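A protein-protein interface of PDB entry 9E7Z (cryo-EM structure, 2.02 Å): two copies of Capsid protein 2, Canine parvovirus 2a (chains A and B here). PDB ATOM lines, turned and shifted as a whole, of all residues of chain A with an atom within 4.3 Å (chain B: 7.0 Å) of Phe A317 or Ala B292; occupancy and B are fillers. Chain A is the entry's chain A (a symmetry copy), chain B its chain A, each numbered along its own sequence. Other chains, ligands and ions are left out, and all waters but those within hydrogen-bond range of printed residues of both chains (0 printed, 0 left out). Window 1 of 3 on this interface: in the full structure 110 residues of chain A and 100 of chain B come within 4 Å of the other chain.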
ATOM      1  N   ALA A  61     -13.339  -7.687  23.237  1.00  0.00           N
ATOM      2  CA  ALA A  61     -14.140  -6.605  22.678  1.00  0.00           C
ATOM      3  C   ALA A  61     -13.282  -5.506  22.059  1.00  0.00           C
ATOM      4  O   ALA A  61     -13.816  -4.653  21.342  1.00  0.00           O
ATOM      5  CB  ALA A  61     -15.044  -6.003  23.755  1.00  0.00           C
ATOM      6  N   ASP A  63     -10.966  -5.980  19.825  1.00  0.00           N
ATOM      7  CA  ASP A  63     -10.392  -6.474  18.582  1.00  0.00           C
ATOM      8  C   ASP A  63     -10.490  -5.419  17.487  1.00  0.00           C
ATOM      9  O   ASP A  63     -11.567  -4.875  17.229  1.00  0.00           O
ATOM     10  CB  ASP A  63     -11.113  -7.749  18.153  1.00  0.00           C
ATOM     11  CG  ASP A  63     -10.457  -8.416  16.967  1.00  0.00           C
ATOM     12  OD1 ASP A  63      -9.224  -8.291  16.825  1.00  0.00           O
ATOM     13  OD2 ASP A  63     -11.173  -9.060  16.179  1.00  0.00           O
ATOM     14  N   SER A 308     -24.146  -8.346  23.916  1.00  0.00           N
ATOM     15  CA  SER A 308     -23.888  -9.641  23.314  1.00  0.00           C
ATOM     16  C   SER A 308     -22.950  -9.456  22.131  1.00  0.00           C
ATOM     17  O   SER A 308     -23.142  -8.551  21.312  1.00  0.00           O
ATOM     18  CB  SER A 308     -25.198 -10.285  22.863  1.00  0.00           C
ATOM     19  OG  SER A 308     -24.982 -11.238  21.841  1.00  0.00           O
ATOM     20  N   PHE A 309     -21.931 -10.297  22.049  1.00  0.00           N
ATOM     21  CA  PHE A 309     -20.975 -10.259  20.952  1.00  0.00           C
ATOM     22  C   PHE A 309     -21.080 -11.557  20.169  1.00  0.00           C
ATOM     23  O   PHE A 309     -20.740 -12.627  20.685  1.00  0.00           O
ATOM     24  CB  PHE A 309     -19.554 -10.043  21.470  1.00  0.00           C
ATOM     25  CG  PHE A 309     -19.279  -8.632  21.895  1.00  0.00           C
ATOM     26  CD1 PHE A 309     -19.630  -8.194  23.160  1.00  0.00           C
ATOM     27  CD2 PHE A 309     -18.682  -7.738  21.023  1.00  0.00           C
ATOM     28  CE1 PHE A 309     -19.385  -6.895  23.549  1.00  0.00           C
ATOM     29  CE2 PHE A 309     -18.433  -6.439  21.406  1.00  0.00           C
ATOM     30  CZ  PHE A 309     -18.785  -6.015  22.672  1.00  0.00           C
ATOM     31  N   GLU A 310     -21.558 -11.459  18.936  1.00  0.00           N
ATOM     32  CA  GLU A 310     -21.645 -12.593  18.033  1.00  0.00           C
ATOM     33  C   GLU A 310     -20.401 -12.646  17.156  1.00  0.00           C
ATOM     34  O   GLU A 310     -19.801 -11.617  16.835  1.00  0.00           O
ATOM     35  CB  GLU A 310     -22.895 -12.503  17.158  1.00  0.00           C
ATOM     36  CG  GLU A 310     -24.199 -12.617  17.922  1.00  0.00           C
ATOM     37  CD  GLU A 310     -25.406 -12.346  17.045  1.00  0.00           C
ATOM     38  OE1 GLU A 310     -25.777 -13.237  16.254  1.00  0.00           O
ATOM     39  OE2 GLU A 310     -25.979 -11.244  17.143  1.00  0.00           O
ATOM     40  N   SER A 312     -18.521 -14.226  13.575  1.00  0.00           N
ATOM     41  CA  SER A 312     -18.706 -14.738  12.225  1.00  0.00           C
ATOM     42  C   SER A 312     -17.312 -14.853  11.611  1.00  0.00           C
ATOM     43  O   SER A 312     -16.293 -14.858  12.311  1.00  0.00           O
ATOM     44  CB  SER A 312     -19.666 -13.848  11.425  1.00  0.00           C
ATOM     45  OG  SER A 312     -20.145 -14.527  10.280  1.00  0.00           O
ATOM     46  N   GLY A 315     -14.645 -12.308  12.740  1.00  0.00           N
ATOM     47  CA  GLY A 315     -14.415 -12.097  14.150  1.00  0.00           C
ATOM     48  C   GLY A 315     -15.612 -11.486  14.852  1.00  0.00           C
ATOM     49  O   GLY A 315     -16.662 -11.253  14.249  1.00  0.00           O
ATOM     50  N   PRO A 316     -15.469 -11.210  16.147  1.00  0.00           N
ATOM     51  CA  PRO A 316     -16.623 -10.769  16.938  1.00  0.00           C
ATOM     52  C   PRO A 316     -17.091  -9.367  16.575  1.00  0.00           C
ATOM     53  O   PRO A 316     -16.310  -8.507  16.166  1.00  0.00           O
ATOM     54  CB  PRO A 316     -16.102 -10.820  18.377  1.00  0.00           C
ATOM     55  CG  PRO A 316     -14.637 -10.633  18.249  1.00  0.00           C
ATOM     56  CD  PRO A 316     -14.241 -11.282  16.955  1.00  0.00           C
ATOM     57  N   PHE A 317     -18.393  -9.151  16.740  1.00  0.00           N
ATOM     58  CA  PHE A 317     -19.006  -7.840  16.604  1.00  0.00           C
ATOM     59  C   PHE A 317     -20.171  -7.747  17.578  1.00  0.00           C
ATOM     60  O   PHE A 317     -20.799  -8.754  17.911  1.00  0.00           O
ATOM     61  CB  PHE A 317     -19.492  -7.582  15.171  1.00  0.00           C
ATOM     62  CG  PHE A 317     -20.427  -8.637  14.651  1.00  0.00           C
ATOM     63  CD1 PHE A 317     -21.788  -8.549  14.883  1.00  0.00           C
ATOM     64  CD2 PHE A 317     -19.941  -9.717  13.936  1.00  0.00           C
ATOM     65  CE1 PHE A 317     -22.650  -9.519  14.409  1.00  0.00           C
ATOM     66  CE2 PHE A 317     -20.795 -10.689  13.460  1.00  0.00           C
ATOM     67  CZ  PHE A 317     -22.154 -10.589  13.696  1.00  0.00           C
ATOM     68  N   LYS A 318     -20.458  -6.530  18.030  1.00  0.00           N
ATOM     69  CA  LYS A 318     -21.543  -6.340  18.982  1.00  0.00           C
ATOM     70  C   LYS A 318     -22.893  -6.476  18.293  1.00  0.00           C
ATOM     71  O   LYS A 318     -23.078  -6.034  17.157  1.00  0.00           O
ATOM     72  CB  LYS A 318     -21.441  -4.971  19.653  1.00  0.00           C
ATOM     73  CG  LYS A 318     -22.304  -4.849  20.903  1.00  0.00           C
ATOM     74  CD  LYS A 318     -22.392  -3.420  21.412  1.00  0.00           C
ATOM     75  CE  LYS A 318     -23.407  -2.607  20.630  1.00  0.00           C
ATOM     76  NZ  LYS A 318     -24.809  -2.908  21.034  1.00  0.00           N
ATOM     77  N   THR A 319     -23.839  -7.086  18.991  1.00  0.00           N
ATOM     78  CA  THR A 319     -25.194  -7.216  18.478  1.00  0.00           C
ATOM     79  C   THR A 319     -25.893  -5.862  18.547  1.00  0.00           C
ATOM     80  O   THR A 319     -26.056  -5.319  19.650  1.00  0.00           O
ATOM     81  CB  THR A 319     -25.975  -8.250  19.291  1.00  0.00           C
ATOM     82  OG1 THR A 319     -25.250  -9.485  19.328  1.00  0.00           O
ATOM     83  CG2 THR A 319     -27.354  -8.487  18.684  1.00  0.00           C
ATOM     84  N   THR B 245     -19.502  -9.737   6.635  1.00  0.00           N
ATOM     85  CA  THR B 245     -20.172  -9.749   7.922  1.00  0.00           C
ATOM     86  C   THR B 245     -20.260  -8.320   8.459  1.00  0.00           C
ATOM     87  O   THR B 245     -19.898  -7.353   7.786  1.00  0.00           O
ATOM     88  CB  THR B 245     -19.434 -10.654   8.908  1.00  0.00           C
ATOM     89  OG1 THR B 245     -18.195 -10.045   9.290  1.00  0.00           O
ATOM     90  CG2 THR B 245     -19.162 -12.017   8.288  1.00  0.00           C
ATOM     91  N   ASN B 246     -20.740  -8.191   9.693  1.00  0.00           N
ATOM     92  CA  ASN B 246     -20.838  -6.882  10.328  1.00  0.00           C
ATOM     93  C   ASN B 246     -19.477  -6.202  10.402  1.00  0.00           C
ATOM     94  O   ASN B 246     -19.391  -4.972  10.365  1.00  0.00           O
ATOM     95  CB  ASN B 246     -21.433  -7.007  11.732  1.00  0.00           C
ATOM     96  CG  ASN B 246     -22.929  -6.798  11.745  1.00  0.00           C
ATOM     97  OD1 ASN B 246     -23.669  -7.516  11.079  1.00  0.00           O
ATOM     98  ND2 ASN B 246     -23.383  -5.805  12.500  1.00  0.00           N
ATOM     99  N   ARG B 247     -18.410  -6.998  10.497  1.00  0.00           N
ATOM    100  CA  ARG B 247     -17.072  -6.447  10.680  1.00  0.00           C
ATOM    101  C   ARG B 247     -16.528  -5.786   9.418  1.00  0.00           C
ATOM    102  O   ARG B 247     -15.569  -5.013   9.507  1.00  0.00           O
ATOM    103  CB  ARG B 247     -16.118  -7.552  11.138  1.00  0.00           C
ATOM    104  CG  ARG B 247     -16.217  -7.902  12.618  1.00  0.00           C
ATOM    105  CD  ARG B 247     -15.605  -6.819  13.499  1.00  0.00           C
ATOM    106  NE  ARG B 247     -14.151  -6.763  13.382  1.00  0.00           N
ATOM    107  CZ  ARG B 247     -13.302  -7.397  14.178  1.00  0.00           C
ATOM    108  NH1 ARG B 247     -13.720  -8.156  15.176  1.00  0.00           N
ATOM    109  NH2 ARG B 247     -11.996  -7.265  13.965  1.00  0.00           N
ATOM    110  N   MET B 283     -22.785   1.763  22.264  1.00  0.00           N
ATOM    111  CA  MET B 283     -22.495   1.524  23.675  1.00  0.00           C
ATOM    112  C   MET B 283     -22.336   2.882  24.353  1.00  0.00           C
ATOM    113  O   MET B 283     -21.268   3.491  24.362  1.00  0.00           O
ATOM    114  CB  MET B 283     -21.252   0.652  23.814  1.00  0.00           C
ATOM    115  CG  MET B 283     -21.318  -0.622  22.981  1.00  0.00           C
ATOM    116  SD  MET B 283     -19.865  -1.671  23.136  1.00  0.00           S
ATOM    117  CE  MET B 283     -19.953  -2.110  24.866  1.00  0.00           C
ATOM    118  N   ILE B 289     -13.836   2.747  21.010  1.00  0.00           N
ATOM    119  CA  ILE B 289     -14.276   2.539  19.638  1.00  0.00           C
ATOM    120  C   ILE B 289     -13.303   1.556  19.005  1.00  0.00           C
ATOM    121  O   ILE B 289     -12.124   1.873  18.804  1.00  0.00           O
ATOM    122  CB  ILE B 289     -14.347   3.849  18.842  1.00  0.00           C
ATOM    123  CG1 ILE B 289     -15.163   4.896  19.606  1.00  0.00           C
ATOM    124  CG2 ILE B 289     -14.958   3.601  17.467  1.00  0.00           C
ATOM    125  CD1 ILE B 289     -15.383   6.180  18.835  1.00  0.00           C
ATOM    126  N   THR B 290     -13.798   0.365  18.694  1.00  0.00           N
ATOM    127  CA  THR B 290     -13.021  -0.686  18.062  1.00  0.00           C
ATOM    128  C   THR B 290     -13.848  -1.285  16.937  1.00  0.00           C
ATOM    129  O   THR B 290     -15.026  -0.964  16.765  1.00  0.00           O
ATOM    130  CB  THR B 290     -12.620  -1.774  19.069  1.00  0.00           C
ATOM    131  OG1 THR B 290     -13.758  -2.592  19.370  1.00  0.00           O
ATOM    132  CG2 THR B 290     -12.092  -1.153  20.353  1.00  0.00           C
ATOM    133  N   GLU B 291     -13.221  -2.167  16.159  1.00  0.00           N
ATOM    134  CA  GLU B 291     -13.961  -2.846  15.103  1.00  0.00           C
ATOM    135  C   GLU B 291     -15.086  -3.694  15.676  1.00  0.00           C
ATOM    136  O   GLU B 291     -16.111  -3.895  15.017  1.00  0.00           O
ATOM    137  CB  GLU B 291     -13.011  -3.700  14.266  1.00  0.00           C
ATOM    138  CG  GLU B 291     -12.016  -2.882  13.463  1.00  0.00           C
ATOM    139  CD  GLU B 291     -12.690  -1.849  12.579  1.00  0.00           C
ATOM    140  OE1 GLU B 291     -13.294  -2.236  11.558  1.00  0.00           O
ATOM    141  OE2 GLU B 291     -12.640  -0.652  12.922  1.00  0.00           O
ATOM    142  N   ALA B 292     -14.921  -4.189  16.904  1.00  0.00           N
ATOM    143  CA  ALA B 292     -15.972  -4.984  17.525  1.00  0.00           C
ATOM    144  C   ALA B 292     -17.122  -4.110  18.011  1.00  0.00           C
ATOM    145  O   ALA B 292     -18.285  -4.529  17.963  1.00  0.00           O
ATOM    146  CB  ALA B 292     -15.395  -5.800  18.680  1.00  0.00           C
ATOM    147  N   THR B 293     -16.826  -2.897  18.480  1.00  0.00           N
ATOM    148  CA  THR B 293     -17.827  -2.063  19.136  1.00  0.00           C
ATOM    149  C   THR B 293     -18.375  -0.942  18.265  1.00  0.00           C
ATOM    150  O   THR B 293     -19.359  -0.310  18.658  1.00  0.00           O
ATOM    151  CB  THR B 293     -17.251  -1.433  20.412  1.00  0.00           C
ATOM    152  OG1 THR B 293     -16.161  -0.566  20.073  1.00  0.00           O
ATOM    153  CG2 THR B 293     -16.773  -2.507  21.377  1.00  0.00           C
ATOM    154  N   ILE B 294     -17.774  -0.668  17.106  1.00  0.00           N
ATOM    155  CA  ILE B 294     -18.233   0.455  16.302  1.00  0.00           C
ATOM    156  C   ILE B 294     -19.600   0.138  15.711  1.00  0.00           C
ATOM    157  O   ILE B 294     -19.891  -1.004  15.334  1.00  0.00           O
ATOM    158  CB  ILE B 294     -17.212   0.800  15.204  1.00  0.00           C
ATOM    159  CG1 ILE B 294     -17.536   2.174  14.607  1.00  0.00           C
ATOM    160  CG2 ILE B 294     -17.193  -0.275  14.122  1.00  0.00           C
ATOM    161  CD1 ILE B 294     -16.454   2.735  13.723  1.00  0.00           C
ATOM    162  N   MET B 295     -20.451   1.159  15.642  1.00  0.00           N
ATOM    163  CA  MET B 295     -21.801   0.981  15.127  1.00  0.00           C
ATOM    164  C   MET B 295     -21.768   0.556  13.665  1.00  0.00           C
ATOM    165  O   MET B 295     -21.048   1.138  12.851  1.00  0.00           O
ATOM    166  CB  MET B 295     -22.593   2.282  15.277  1.00  0.00           C
ATOM    167  CG  MET B 295     -24.021   2.219  14.740  1.00  0.00           C
ATOM    168  SD  MET B 295     -24.837   3.827  14.742  1.00  0.00           S
ATOM    169  CE  MET B 295     -25.422   3.903  16.430  1.00  0.00           C
ATOM    170  N   ARG B 296     -22.553  -0.457  13.341  1.00  0.00           N
ATOM    171  CA  ARG B 296     -22.776  -0.881  11.971  1.00  0.00           C
ATOM    172  C   ARG B 296     -24.242  -0.661  11.606  1.00  0.00           C
ATOM    173  O   ARG B 296     -25.102  -0.630  12.491  1.00  0.00           O
ATOM    174  CB  ARG B 296     -22.410  -2.359  11.776  1.00  0.00           C
ATOM    175  CG  ARG B 296     -21.062  -2.771  12.379  1.00  0.00           C
ATOM    176  CD  ARG B 296     -19.873  -2.149  11.648  1.00  0.00           C
ATOM    177  NE  ARG B 296     -18.595  -2.616  12.179  1.00  0.00           N
ATOM    178  CZ  ARG B 296     -17.436  -2.537  11.539  1.00  0.00           C
ATOM    179  NH1 ARG B 296     -17.345  -2.011  10.329  1.00  0.00           N
ATOM    180  NH2 ARG B 296     -16.335  -2.993  12.132  1.00  0.00           N
ATOM    181  N   ALA B 298     -26.700  -2.392  10.409  1.00  0.00           N
ATOM    182  CA  ALA B 298     -27.636  -3.433  10.811  1.00  0.00           C
ATOM    183  C   ALA B 298     -26.824  -4.687  11.116  1.00  0.00           C
ATOM    184  O   ALA B 298     -25.598  -4.631  11.246  1.00  0.00           O
ATOM    185  CB  ALA B 298     -28.695  -3.664   9.728  1.00  0.00           C
ATOM    186  N   GLU B 299     -27.505  -5.822  11.229  1.00  0.00           N
ATOM    187  CA  GLU B 299     -26.858  -7.098  11.503  1.00  0.00           C
ATOM    188  C   GLU B 299     -27.008  -8.017  10.298  1.00  0.00           C
ATOM    189  O   GLU B 299     -28.124  -8.233   9.812  1.00  0.00           O
ATOM    190  CB  GLU B 299     -27.441  -7.759  12.751  1.00  0.00           C
ATOM    191  CG  GLU B 299     -26.616  -8.942  13.235  1.00  0.00           C
ATOM    192  CD  GLU B 299     -27.021  -9.427  14.610  1.00  0.00           C
ATOM    193  OE1 GLU B 299     -27.628  -8.640  15.365  1.00  0.00           O
ATOM    194  OE2 GLU B 299     -26.731 -10.594  14.937  1.00  0.00           O
ATOM    195  N   VAL B 300     -25.890  -8.558   9.828  1.00  0.00           N
ATOM    196  CA  VAL B 300     -25.913  -9.579   8.787  1.00  0.00           C
ATOM    197  C   VAL B 300     -25.955 -10.940   9.466  1.00  0.00           C
ATOM    198  O   VAL B 300     -25.045 -11.297  10.221  1.00  0.00           O
ATOM    199  CB  VAL B 300     -24.695  -9.455   7.859  1.00  0.00           C
ATOM    200  CG1 VAL B 300     -24.733 -10.536   6.787  1.00  0.00           C
ATOM    201  CG2 VAL B 300     -24.647  -8.071   7.229  1.00  0.00           C
ATOM    202  N   GLY B 301     -27.015 -11.697   9.207  1.00  0.00           N
ATOM    203  CA  GLY B 301     -27.201 -12.981   9.852  1.00  0.00           C
ATOM    204  C   GLY B 301     -27.812 -12.837  11.235  1.00  0.00           C
ATOM    205  O   GLY B 301     -28.089 -11.746  11.728  1.00  0.00           O
ATOM    206  N   GLY B 371     -23.574 -16.860   8.264  1.00  0.00           N
ATOM    207  CA  GLY B 371     -23.739 -17.734   9.402  1.00  0.00           C
ATOM    208  C   GLY B 371     -23.054 -17.199  10.644  1.00  0.00           C
ATOM    209  O   GLY B 371     -22.657 -16.036  10.733  1.00  0.00           O
ATOM    210  N   ARG B 372     -22.910 -18.086  11.624  1.00  0.00           N
ATOM    211  CA  ARG B 372     -22.350 -17.737  12.919  1.00  0.00           C
ATOM    212  C   ARG B 372     -21.310 -18.764  13.338  1.00  0.00           C
ATOM    213  O   ARG B 372     -21.323 -19.910  12.888  1.00  0.00           O
ATOM    214  CB  ARG B 372     -23.439 -17.648  13.997  1.00  0.00           C
ATOM    215  CG  ARG B 372     -24.323 -16.422  13.888  1.00  0.00           C
ATOM    216  CD  ARG B 372     -23.575 -15.158  14.265  1.00  0.00           C
ATOM    217  NE  ARG B 372     -24.413 -13.970  14.167  1.00  0.00           N
ATOM    218  CZ  ARG B 372     -24.642 -13.301  13.045  1.00  0.00           C
ATOM    219  NH1 ARG B 372     -24.137 -13.695  11.886  1.00  0.00           N
ATOM    220  NH2 ARG B 372     -25.398 -12.209  13.085  1.00  0.00           N
ATOM    221  N   GLY B 376     -17.169 -18.304  19.184  1.00  0.00           N
ATOM    222  CA  GLY B 376     -16.660 -16.957  19.300  1.00  0.00           C
ATOM    223  C   GLY B 376     -17.605 -15.956  19.928  1.00  0.00           C
ATOM    224  O   GLY B 376     -17.232 -14.790  20.077  1.00  0.00           O
ATOM    225  N   TRP B 378     -19.970 -14.175  22.962  1.00  0.00           N
ATOM    226  CA  TRP B 378     -19.964 -14.019  24.411  1.00  0.00           C
ATOM    227  C   TRP B 378     -20.929 -12.913  24.810  1.00  0.00           C
ATOM    228  O   TRP B 378     -21.272 -12.036  24.014  1.00  0.00           O
ATOM    229  CB  TRP B 378     -18.558 -13.729  24.956  1.00  0.00           C
ATOM    230  CG  TRP B 378     -18.058 -12.338  24.713  1.00  0.00           C
ATOM    231  CD1 TRP B 378     -18.186 -11.264  25.545  1.00  0.00           C
ATOM    232  CD2 TRP B 378     -17.329 -11.874  23.571  1.00  0.00           C
ATOM    233  NE1 TRP B 378     -17.589 -10.160  24.989  1.00  0.00           N
ATOM    234  CE2 TRP B 378     -17.056 -10.506  23.776  1.00  0.00           C
ATOM    235  CE3 TRP B 378     -16.885 -12.480  22.391  1.00  0.00           C
ATOM    236  CZ2 TRP B 378     -16.361  -9.735  22.846  1.00  0.00           C
ATOM    237  CZ3 TRP B 378     -16.195 -11.712  21.469  1.00  0.00           C
ATOM    238  CH2 TRP B 378     -15.940 -10.355  21.702  1.00  0.00           C
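NH1 of Arg B247 is in salt-bridge range of OD2 of Asp A63, at 2.9 Å.
The backbone carbonyl oxygen (O) of Gly B371 sits at hydrogen-bond distance from the side-chain hydroxyl (OG) of Ser A312.
NE of Arg B372 is in salt-bridge range of OE1 of Glu A310 (2.6 Å).
The side-chain hydroxyl (OG1) of Thr B290 is in hydrogen-bond range of the backbone carbonyl oxygen (O) of Ala A61 (2.9 Å).
The guanidinium group of Arg B247 is in hydrogen-bond range of the backbone carbonyl oxygen of Pro A316 (2.8 Å).
N of Ala B292 sits at hydrogen-bond distance from O of Asp A63 (3.4 Å).
OE2 of Glu A310 sits close to OE2 of Glu B299 (2.4 Å).
The backbone carbonyl oxygen (O) of Trp B378 sits at hydrogen-bond distance from the backbone NH (N) of Phe A309, at 2.7 Å.
O of Ala B292 sits at hydrogen-bond distance from N of Lys A318, at 3.0 Å.
O of Asp A63 sits at hydrogen-bond distance from N of Glu B291.
O of Ser A308 is in hydrogen-bond range of N of Thr A319, 2.8 Å away.
The backbone carbonyl oxygen (O) of Glu A310 lies within hydrogen-bond range of the backbone NH (N) of Phe A317, 2.8 Å away.
OG1 of Thr B245 sits close to N of Arg B247, 3.3 Å away.
OG1 of Thr B290 sits close to N of Ala B292 (3.2 Å).
The backbone carbonyl oxygen of Asn B246 sits at hydrogen-bond distance from the guanidinium group of Arg B296 (3.1 Å).
The backbone carbonyl oxygen (O) of Val B300 lies within hydrogen-bond range of the guanidinium group (NH2) of Arg B372 (3.0 Å).
Among the printed residues, merely in contact across the chains: Pro A316 with Trp B378, Ala A61 with Ala B292, Thr A319 with Glu B299, Ser A312 with Thr B245, Lys A318 with Met B283, Phe A317 with Asn B246, Ser A308 with Trp B378, Phe A317 with Ala B292, Ala A61 with Thr B293, Ala A61 with Trp B378, Phe A317 with Arg B372, Gly A315 with Arg B247, Asp A63 with Thr B290, Pro A316 with Ala B292 and Phe A309 with Ala B292.
Phe A317 touches just these residues of chain B: Asn B246 (3.5 Å), Ala B292 (3.7 Å) and Arg B372 (3.7 Å).
Of the printed residues of chain B, Asp A63 touches Arg B247 (2.9 Å), Thr B290 (3.8 Å), Glu B291 (3.3 Å) and Ala B292 (3.4 Å).
Printed residues of chain B within 4 Å of Ser A308: Trp B378 (3.6 Å).
Of the printed residues of chain A, Arg B247 touches Asp A63, Gly A315 and Pro A316.
Of the printed residues of chain A, Gly B371 touches Ser A312 (3.0 Å).
Printed residues of chain B within 4 Å of Gly A315: Arg B247.
The nearest printed residue of chain A that does not touch Ala B292 is Thr A319 (6.2 Å).
Of the 20 printed residues of chain B, 12 touch a printed residue of chain A.
Printed residues of chain A that touch a printed residue of chain B: Ala A61, Asp A63, Ser A308, Phe A309, Glu A310, Ser A312, Gly A315, Pro A316, Phe A317, Lys A318 and Thr A319.
Among the printed residues, Asp or Glu carboxylates within 4 Å of a Lys or Arg side-chain nitrogen of the other chain: Asp A63 with Arg B247 and Glu A310 with Arg B372.
No position is printed for both chains.
Of the 25 pairs that touch across the chains among the printed residues, none has its exchanged pair printed and touching as well.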
